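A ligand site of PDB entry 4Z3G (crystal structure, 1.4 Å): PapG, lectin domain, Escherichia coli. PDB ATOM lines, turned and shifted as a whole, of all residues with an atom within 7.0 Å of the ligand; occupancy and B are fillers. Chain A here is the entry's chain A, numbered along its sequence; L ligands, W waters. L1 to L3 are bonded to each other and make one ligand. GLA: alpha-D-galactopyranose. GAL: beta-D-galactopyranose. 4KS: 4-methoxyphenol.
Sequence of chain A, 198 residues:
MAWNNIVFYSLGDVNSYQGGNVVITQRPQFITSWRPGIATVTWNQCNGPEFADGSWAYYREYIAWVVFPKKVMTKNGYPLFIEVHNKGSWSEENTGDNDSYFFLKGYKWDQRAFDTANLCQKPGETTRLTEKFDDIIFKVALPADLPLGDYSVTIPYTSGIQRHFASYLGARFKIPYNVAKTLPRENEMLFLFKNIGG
The backbone carbonyl oxygen (O) of Lys 105 sits at hydrogen-bond distance from the backbone NH (N) of Ala 64 (2.9 Å).
OE1 of Glu 93 lies within salt-bridge range of NZ of Lys 174 (2.8 Å).
The side-chain carboxylate of Glu 93 sits at hydrogen-bond distance from the side-chain hydroxyl of Ser 91, at 2.7 Å.
The side-chain carboxylate (OE2) of Glu 61 is in hydrogen-bond range of the backbone NH (N) of Phe 173, 2.9 Å away.
The side-chain hydroxyl of Tyr 177 sits at hydrogen-bond distance from the side-chain carboxylate of Glu 93 (2.7 Å).
OD1 of Asp 110 lies within salt-bridge range of NH1 of Arg 172, 2.8 Å away.
N of Leu 104 is in hydrogen-bond range of O of Ser 91 (2.8 Å).
NZ of Lys 105 sits at hydrogen-bond distance from O of Ser 89.
The side-chain carboxylate (OE1) of Glu 61 lies within hydrogen-bond range of an oxygen (O6) of GAL L2 (2.6 Å).
O of Gly 106 lies within hydrogen-bond range of O3 of GAL L2.
NZ of Lys 174 sits at hydrogen-bond distance from O3 of GLA L1, at 2.9 Å.
OE2 of Glu 93 sits at hydrogen-bond distance from O4 of GLA L1 (2.7 Å).
The backbone NH (N) of Gly 106 is in hydrogen-bond range of an oxygen (O6) of GLA L1 (2.7 Å).
Water W5 bridges O6 of GLA L1 and NZ of Lys 105.
Water W2 lies within hydrogen-bond range of an oxygen (O6) of GAL L2 (2.7 Å), the backbone carbonyl oxygen (O) of Lys 108 (2.9 Å), the backbone carbonyl oxygen (O) of Tyr 62 (3.0 Å) and the backbone NH (N) of Tyr 107 (3.3 Å).
Water W3 lies within hydrogen-bond range of OE1 of Glu 61, O2 of GLA L1 and O of Phe 173.
CB of Ser 91 touches C6 of GLA L1, at 3.7 Å.
Leu 104 touches the ligand.
CA of Lys 105 touches O6 of GLA L1 (3.5 Å).
NE1 of Trp 109 touches C5 of 4KS L3 (3.3 Å).
Arg 172 touches the ligand.
Hydrophobic or aromatic side chains that line the ligand: Leu 104 and Trp 109.
Of the 20 residues printed, 9 come within 4 Å of the ligand.
The nearest printed residue that does not touch the ligand is Ile 63 (4.2 Å).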
ATOM      1  N   GLU A  61       7.936 -16.092 -29.907  1.00  0.00           N
ATOM      2  CA  GLU A  61       7.792 -14.749 -29.355  1.00  0.00           C
ATOM      3  C   GLU A  61       9.150 -14.082 -29.574  1.00  0.00           C
ATOM      4  O   GLU A  61      10.164 -14.576 -29.044  1.00  0.00           O
ATOM      5  CB  GLU A  61       7.443 -14.735 -27.855  1.00  0.00           C
ATOM      6  CG  GLU A  61       7.345 -13.332 -27.274  1.00  0.00           C
ATOM      7  CD  GLU A  61       7.345 -13.251 -25.749  1.00  0.00           C
ATOM      8  OE1 GLU A  61       6.621 -12.373 -25.215  1.00  0.00           O
ATOM      9  OE2 GLU A  61       8.099 -14.018 -25.108  1.00  0.00           O
ATOM     10  N   TYR A  62       9.212 -12.998 -30.366  1.00  0.00           N
ATOM     11  CA  TYR A  62      10.485 -12.330 -30.655  1.00  0.00           C
ATOM     12  C   TYR A  62      10.401 -10.884 -30.181  1.00  0.00           C
ATOM     13  O   TYR A  62       9.401 -10.205 -30.420  1.00  0.00           O
ATOM     14  CB  TYR A  62      10.845 -12.322 -32.152  1.00  0.00           C
ATOM     15  CG  TYR A  62      11.037 -13.644 -32.869  1.00  0.00           C
ATOM     16  CD1 TYR A  62      11.037 -14.863 -32.187  1.00  0.00           C
ATOM     17  CD2 TYR A  62      11.200 -13.682 -34.248  1.00  0.00           C
ATOM     18  CE1 TYR A  62      11.267 -16.070 -32.850  1.00  0.00           C
ATOM     19  CE2 TYR A  62      11.451 -14.884 -34.917  1.00  0.00           C
ATOM     20  CZ  TYR A  62      11.449 -16.080 -34.229  1.00  0.00           C
ATOM     21  OH  TYR A  62      11.732 -17.272 -34.867  1.00  0.00           O
ATOM     22  N   ILE A  63      11.473 -10.399 -29.538  1.00  0.00           N
ATOM     23  CA  ILE A  63      11.571  -9.058 -28.992  1.00  0.00           C
ATOM     24  C   ILE A  63      12.943  -8.486 -29.357  1.00  0.00           C
ATOM     25  O   ILE A  63      13.961  -9.081 -29.011  1.00  0.00           O
ATOM     26  CB  ILE A  63      11.389  -9.017 -27.461  1.00  0.00           C
ATOM     27  CG1 ILE A  63      10.083  -9.694 -27.013  1.00  0.00           C
ATOM     28  CG2 ILE A  63      11.469  -7.559 -26.961  1.00  0.00           C
ATOM     29  CD1 ILE A  63       9.884  -9.717 -25.518  1.00  0.00           C
ATOM     30  N   ALA A  64      12.958  -7.331 -30.032  1.00  0.00           N
ATOM     31  CA  ALA A  64      14.214  -6.637 -30.342  1.00  0.00           C
ATOM     32  C   ALA A  64      14.618  -5.751 -29.174  1.00  0.00           C
ATOM     33  O   ALA A  64      13.753  -5.181 -28.506  1.00  0.00           O
ATOM     34  CB  ALA A  64      14.060  -5.787 -31.580  1.00  0.00           C
ATOM     35  N   SER A  89       8.898   4.256 -32.527  1.00  0.00           N
ATOM     36  CA  SER A  89       7.948   3.302 -31.923  1.00  0.00           C
ATOM     37  C   SER A  89       8.568   2.479 -30.781  1.00  0.00           C
ATOM     38  O   SER A  89       7.876   1.687 -30.153  1.00  0.00           O
ATOM     39  CB  SER A  89       7.431   2.320 -32.968  1.00  0.00           C
ATOM     40  OG  SER A  89       8.496   1.571 -33.537  1.00  0.00           O
ATOM     41  N   TRP A  90       9.870   2.630 -30.517  1.00  0.00           N
ATOM     42  CA  TRP A  90      10.510   1.817 -29.498  1.00  0.00           C
ATOM     43  C   TRP A  90       9.893   2.021 -28.111  1.00  0.00           C
ATOM     44  O   TRP A  90       9.504   3.134 -27.777  1.00  0.00           O
ATOM     45  CB  TRP A  90      12.017   2.128 -29.436  1.00  0.00           C
ATOM     46  CG  TRP A  90      12.819   1.625 -30.604  1.00  0.00           C
ATOM     47  CD1 TRP A  90      13.200   2.328 -31.718  1.00  0.00           C
ATOM     48  CD2 TRP A  90      13.419   0.334 -30.715  1.00  0.00           C
ATOM     49  NE1 TRP A  90      13.966   1.536 -32.531  1.00  0.00           N
ATOM     50  CE2 TRP A  90      14.153   0.314 -31.925  1.00  0.00           C
ATOM     51  CE3 TRP A  90      13.336  -0.852 -29.974  1.00  0.00           C
ATOM     52  CZ2 TRP A  90      14.834  -0.818 -32.371  1.00  0.00           C
ATOM     53  CZ3 TRP A  90      14.100  -1.936 -30.358  1.00  0.00           C
ATOM     54  CH2 TRP A  90      14.783  -1.932 -31.577  1.00  0.00           C
ATOM     55  N   SER A  91       9.824   0.945 -27.319  1.00  0.00           N
ATOM     56  CA  SER A  91       9.343   1.001 -25.956  1.00  0.00           C
ATOM     57  C   SER A  91      10.561   1.282 -25.068  1.00  0.00           C
ATOM     58  O   SER A  91      11.466   0.437 -25.016  1.00  0.00           O
ATOM     59  CB  SER A  91       8.697  -0.337 -25.586  1.00  0.00           C
ATOM     60  OG  SER A  91       8.230  -0.293 -24.247  1.00  0.00           O
ATOM     61  N   GLU A  93      12.071   1.448 -21.640  1.00  0.00           N
ATOM     62  CA  GLU A  93      11.698   0.770 -20.395  1.00  0.00           C
ATOM     63  C   GLU A  93      12.751   0.886 -19.316  1.00  0.00           C
ATOM     64  O   GLU A  93      13.873   1.295 -19.592  1.00  0.00           O
ATOM     65  CB  GLU A  93      11.440  -0.712 -20.692  1.00  0.00           C
ATOM     66  CG  GLU A  93      10.382  -0.894 -21.780  1.00  0.00           C
ATOM     67  CD  GLU A  93       9.854  -2.299 -21.991  1.00  0.00           C
ATOM     68  OE1 GLU A  93      10.256  -3.232 -21.253  1.00  0.00           O
ATOM     69  OE2 GLU A  93       9.078  -2.483 -22.960  1.00  0.00           O
ATOM     70  N   LEU A 104      12.934  -1.611 -26.272  1.00  0.00           N
ATOM     71  CA  LEU A 104      12.441  -2.929 -26.655  1.00  0.00           C
ATOM     72  C   LEU A 104      11.360  -2.774 -27.731  1.00  0.00           C
ATOM     73  O   LEU A 104      10.622  -1.774 -27.762  1.00  0.00           O
ATOM     74  CB  LEU A 104      11.841  -3.718 -25.453  1.00  0.00           C
ATOM     75  CG  LEU A 104      12.847  -4.321 -24.449  1.00  0.00           C
ATOM     76  CD1 LEU A 104      13.492  -3.244 -23.562  1.00  0.00           C
ATOM     77  CD2 LEU A 104      12.172  -5.355 -23.573  1.00  0.00           C
ATOM     78  N   LYS A 105      11.225  -3.800 -28.561  1.00  0.00           N
ATOM     79  CA  LYS A 105      10.124  -3.871 -29.508  1.00  0.00           C
ATOM     80  C   LYS A 105       9.706  -5.308 -29.651  1.00  0.00           C
ATOM     81  O   LYS A 105      10.386  -6.073 -30.328  1.00  0.00           O
ATOM     82  CB  LYS A 105      10.440  -3.218 -30.870  1.00  0.00           C
ATOM     83  CG  LYS A 105       9.258  -3.288 -31.846  1.00  0.00           C
ATOM     84  CD  LYS A 105       7.924  -2.760 -31.310  1.00  0.00           C
ATOM     85  CE  LYS A 105       8.012  -1.319 -30.852  1.00  0.00           C
ATOM     86  NZ  LYS A 105       6.726  -0.790 -30.330  1.00  0.00           N
ATOM     87  N   GLY A 106       8.585  -5.659 -29.037  1.00  0.00           N
ATOM     88  CA  GLY A 106       8.026  -6.992 -29.156  1.00  0.00           C
ATOM     89  C   GLY A 106       7.177  -6.990 -30.389  1.00  0.00           C
ATOM     90  O   GLY A 106       6.163  -6.282 -30.417  1.00  0.00           O
ATOM     91  N   TYR A 107       7.594  -7.750 -31.423  1.00  0.00           N
ATOM     92  CA  TYR A 107       6.934  -7.737 -32.733  1.00  0.00           C
ATOM     93  C   TYR A 107       6.321  -9.056 -33.176  1.00  0.00           C
ATOM     94  O   TYR A 107       5.727  -9.129 -34.269  1.00  0.00           O
ATOM     95  CB  TYR A 107       7.944  -7.207 -33.777  1.00  0.00           C
ATOM     96  CG  TYR A 107       9.148  -8.110 -33.991  1.00  0.00           C
ATOM     97  CD1 TYR A 107      10.264  -8.032 -33.155  1.00  0.00           C
ATOM     98  CD2 TYR A 107       9.226  -8.966 -35.081  1.00  0.00           C
ATOM     99  CE1 TYR A 107      11.334  -8.903 -33.305  1.00  0.00           C
ATOM    100  CE2 TYR A 107      10.335  -9.778 -35.283  1.00  0.00           C
ATOM    101  CZ  TYR A 107      11.387  -9.742 -34.390  1.00  0.00           C
ATOM    102  OH  TYR A 107      12.489 -10.549 -34.538  1.00  0.00           O
ATOM    103  N   LYS A 108       6.502 -10.113 -32.396  1.00  0.00           N
ATOM    104  CA  LYS A 108       5.977 -11.433 -32.727  1.00  0.00           C
ATOM    105  C   LYS A 108       5.665 -12.142 -31.431  1.00  0.00           C
ATOM    106  O   LYS A 108       6.507 -12.181 -30.539  1.00  0.00           O
ATOM    107  CB  LYS A 108       7.008 -12.234 -33.541  1.00  0.00           C
ATOM    108  CG  LYS A 108       6.534 -13.624 -33.949  1.00  0.00           C
ATOM    109  CD  LYS A 108       7.634 -14.454 -34.620  1.00  0.00           C
ATOM    110  CE  LYS A 108       8.204 -13.863 -35.886  1.00  0.00           C
ATOM    111  NZ  LYS A 108       7.177 -13.516 -36.915  1.00  0.00           N
ATOM    112  N   TRP A 109       4.452 -12.690 -31.316  1.00  0.00           N
ATOM    113  CA  TRP A 109       4.052 -13.412 -30.120  1.00  0.00           C
ATOM    114  C   TRP A 109       2.993 -14.437 -30.453  1.00  0.00           C
ATOM    115  O   TRP A 109       2.228 -14.246 -31.415  1.00  0.00           O
ATOM    116  CB  TRP A 109       3.550 -12.414 -29.059  1.00  0.00           C
ATOM    117  CG  TRP A 109       2.391 -11.581 -29.510  1.00  0.00           C
ATOM    118  CD1 TRP A 109       1.066 -11.873 -29.396  1.00  0.00           C
ATOM    119  CD2 TRP A 109       2.456 -10.301 -30.146  1.00  0.00           C
ATOM    120  NE1 TRP A 109       0.311 -10.905 -30.007  1.00  0.00           N
ATOM    121  CE2 TRP A 109       1.141  -9.901 -30.447  1.00  0.00           C
ATOM    122  CE3 TRP A 109       3.509  -9.479 -30.567  1.00  0.00           C
ATOM    123  CZ2 TRP A 109       0.840  -8.681 -31.042  1.00  0.00           C
ATOM    124  CZ3 TRP A 109       3.212  -8.245 -31.123  1.00  0.00           C
ATOM    125  CH2 TRP A 109       1.897  -7.897 -31.426  1.00  0.00           C
ATOM    126  N   ASP A 110       2.943 -15.548 -29.681  1.00  0.00           N
ATOM    127  CA  ASP A 110       1.906 -16.567 -29.822  1.00  0.00           C
ATOM    128  C   ASP A 110       1.841 -17.125 -31.226  1.00  0.00           C
ATOM    129  O   ASP A 110       0.781 -17.575 -31.647  1.00  0.00           O
ATOM    130  CB  ASP A 110       0.526 -15.990 -29.428  1.00  0.00           C
ATOM    131  CG  ASP A 110       0.443 -15.576 -27.977  1.00  0.00           C
ATOM    132  OD1 ASP A 110       1.251 -16.094 -27.184  1.00  0.00           O
ATOM    133  OD2 ASP A 110      -0.394 -14.686 -27.656  1.00  0.00           O
ATOM    134  N   ALA A 171       2.929 -18.000 -24.359  1.00  0.00           N
ATOM    135  CA  ALA A 171       4.228 -17.960 -23.706  1.00  0.00           C
ATOM    136  C   ALA A 171       4.841 -16.562 -23.782  1.00  0.00           C
ATOM    137  O   ALA A 171       4.803 -15.924 -24.828  1.00  0.00           O
ATOM    138  CB  ALA A 171       5.159 -18.990 -24.326  1.00  0.00           C
ATOM    139  N   ARG A 172       5.361 -16.091 -22.651  1.00  0.00           N
ATOM    140  CA  ARG A 172       5.924 -14.758 -22.491  1.00  0.00           C
ATOM    141  C   ARG A 172       7.213 -14.835 -21.700  1.00  0.00           C
ATOM    142  O   ARG A 172       7.255 -15.483 -20.664  1.00  0.00           O
ATOM    143  CB  ARG A 172       4.964 -13.837 -21.697  1.00  0.00           C
ATOM    144  CG  ARG A 172       3.616 -13.598 -22.320  1.00  0.00           C
ATOM    145  CD  ARG A 172       3.652 -12.593 -23.449  1.00  0.00           C
ATOM    146  NE  ARG A 172       2.316 -12.436 -24.041  1.00  0.00           N
ATOM    147  CZ  ARG A 172       1.817 -13.206 -24.989  1.00  0.00           C
ATOM    148  NH1 ARG A 172       2.504 -14.243 -25.465  1.00  0.00           N
ATOM    149  NH2 ARG A 172       0.589 -12.984 -25.454  1.00  0.00           N
ATOM    150  N   PHE A 173       8.250 -14.152 -22.166  1.00  0.00           N
ATOM    151  CA  PHE A 173       9.502 -14.051 -21.447  1.00  0.00           C
ATOM    152  C   PHE A 173      10.166 -12.748 -21.838  1.00  0.00           C
ATOM    153  O   PHE A 173      10.058 -12.312 -22.987  1.00  0.00           O
ATOM    154  CB  PHE A 173      10.414 -15.237 -21.803  1.00  0.00           C
ATOM    155  CG  PHE A 173      11.712 -15.268 -21.032  1.00  0.00           C
ATOM    156  CD1 PHE A 173      11.782 -15.830 -19.766  1.00  0.00           C
ATOM    157  CD2 PHE A 173      12.847 -14.634 -21.519  1.00  0.00           C
ATOM    158  CE1 PHE A 173      12.982 -15.858 -19.062  1.00  0.00           C
ATOM    159  CE2 PHE A 173      14.038 -14.620 -20.788  1.00  0.00           C
ATOM    160  CZ  PHE A 173      14.098 -15.225 -19.564  1.00  0.00           C
ATOM    161  N   LYS A 174      10.878 -12.142 -20.891  1.00  0.00           N
ATOM    162  CA  LYS A 174      11.703 -10.963 -21.138  1.00  0.00           C
ATOM    163  C   LYS A 174      13.008 -11.188 -20.431  1.00  0.00           C
ATOM    164  O   LYS A 174      13.002 -11.462 -19.244  1.00  0.00           O
ATOM    165  CB  LYS A 174      11.040  -9.680 -20.617  1.00  0.00           C
ATOM    166  CG  LYS A 174       9.719  -9.379 -21.311  1.00  0.00           C
ATOM    167  CD  LYS A 174       9.034  -8.114 -20.780  1.00  0.00           C
ATOM    168  CE  LYS A 174       9.710  -6.862 -21.239  1.00  0.00           C
ATOM    169  NZ  LYS A 174       8.948  -5.652 -20.804  1.00  0.00           N
ATOM    170  N   TYR A 177      16.425  -6.956 -17.187  1.00  0.00           N
ATOM    171  CA  TYR A 177      17.201  -5.780 -17.588  1.00  0.00           C
ATOM    172  C   TYR A 177      18.660  -5.846 -17.143  1.00  0.00           C
ATOM    173  O   TYR A 177      19.534  -5.451 -17.903  1.00  0.00           O
ATOM    174  CB  TYR A 177      16.580  -4.479 -17.061  1.00  0.00           C
ATOM    175  CG  TYR A 177      15.167  -4.235 -17.539  1.00  0.00           C
ATOM    176  CD1 TYR A 177      14.887  -4.062 -18.891  1.00  0.00           C
ATOM    177  CD2 TYR A 177      14.094  -4.284 -16.654  1.00  0.00           C
ATOM    178  CE1 TYR A 177      13.578  -3.828 -19.334  1.00  0.00           C
ATOM    179  CE2 TYR A 177      12.792  -4.033 -17.081  1.00  0.00           C
ATOM    180  CZ  TYR A 177      12.535  -3.817 -18.425  1.00  0.00           C
ATOM    181  OH  TYR A 177      11.226  -3.651 -18.804  1.00  0.00           O
HETATM  182  C1  GLA L   1       6.433  -7.325 -25.416  1.00  0.00           C
HETATM  183  C2  GLA L   1       6.613  -7.357 -23.902  1.00  0.00           C
HETATM  184  C3  GLA L   1       6.121  -6.046 -23.308  1.00  0.00           C
HETATM  185  C4  GLA L   1       6.892  -4.889 -23.916  1.00  0.00           C
HETATM  186  C5  GLA L   1       6.724  -4.924 -25.432  1.00  0.00           C
HETATM  187  C6  GLA L   1       7.579  -3.875 -26.109  1.00  0.00           C
HETATM  188  O2  GLA L   1       5.923  -8.473 -23.346  1.00  0.00           O
HETATM  189  O3  GLA L   1       6.286  -6.033 -21.903  1.00  0.00           O
HETATM  190  O4  GLA L   1       8.275  -4.981 -23.602  1.00  0.00           O
HETATM  191  O5  GLA L   1       7.118  -6.213 -25.960  1.00  0.00           O
HETATM  192  O6  GLA L   1       7.306  -3.797 -27.499  1.00  0.00           O
HETATM  193  C1  GAL L   2       1.775  -7.691 -26.988  1.00  0.00           C
HETATM  194  C2  GAL L   2       2.553  -6.391 -27.084  1.00  0.00           C
HETATM  195  C3  GAL L   2       3.885  -6.659 -27.769  1.00  0.00           C
HETATM  196  C4  GAL L   2       4.631  -7.756 -27.007  1.00  0.00           C
HETATM  197  C5  GAL L   2       3.739  -8.982 -26.880  1.00  0.00           C
HETATM  198  C6  GAL L   2       4.340 -10.130 -26.110  1.00  0.00           C
HETATM  199  O2  GAL L   2       1.831  -5.438 -27.871  1.00  0.00           O
HETATM  200  O3  GAL L   2       4.646  -5.471 -27.926  1.00  0.00           O
HETATM  201  O4  GAL L   2       5.038  -7.281 -25.718  1.00  0.00           O
HETATM  202  O5  GAL L   2       2.511  -8.631 -26.239  1.00  0.00           O
HETATM  203  O6  GAL L   2       5.567 -10.547 -26.719  1.00  0.00           O
HETATM  204  C4  4KS L   3      -0.436  -8.397 -26.401  1.00  0.00           C
HETATM  205  C5  4KS L   3      -0.291  -9.675 -26.985  1.00  0.00           C
HETATM  206  C6  4KS L   3      -1.421 -10.497 -27.164  1.00  0.00           C
HETATM  207  O1  4KS L   3       0.600  -7.469 -26.245  1.00  0.00           O
HETATM  208  C3  4KS L   3      -1.677  -7.931 -25.955  1.00  0.00           C
HETATM  209  C2  4KS L   3      -2.795  -8.769 -26.134  1.00  0.00           C
HETATM  210  C1  4KS L   3      -2.671 -10.025 -26.727  1.00  0.00           C
HETATM  211  O   4KS L   3      -3.862 -10.719 -26.868  1.00  0.00           O
HETATM  212  C   4KS L   3      -3.879 -12.009 -27.445  1.00  0.00           C
HETATM  213  O   HOH W   1       3.468  -2.931 -26.648  1.00  0.00           O
HETATM  214  O   HOH W   2       6.787  -9.736 -28.967  1.00  0.00           O
HETATM  215  O   HOH W   3       7.193 -10.900 -23.078  1.00  0.00           O
HETATM  216  O   HOH W   4       3.110  -8.233 -23.337  1.00  0.00           O
HETATM  217  O   HOH W   5       5.429  -2.031 -28.060  1.00  0.00           O
HETATM  218  O   HOH W   6      -2.245 -14.057 -29.360  1.00  0.00           O
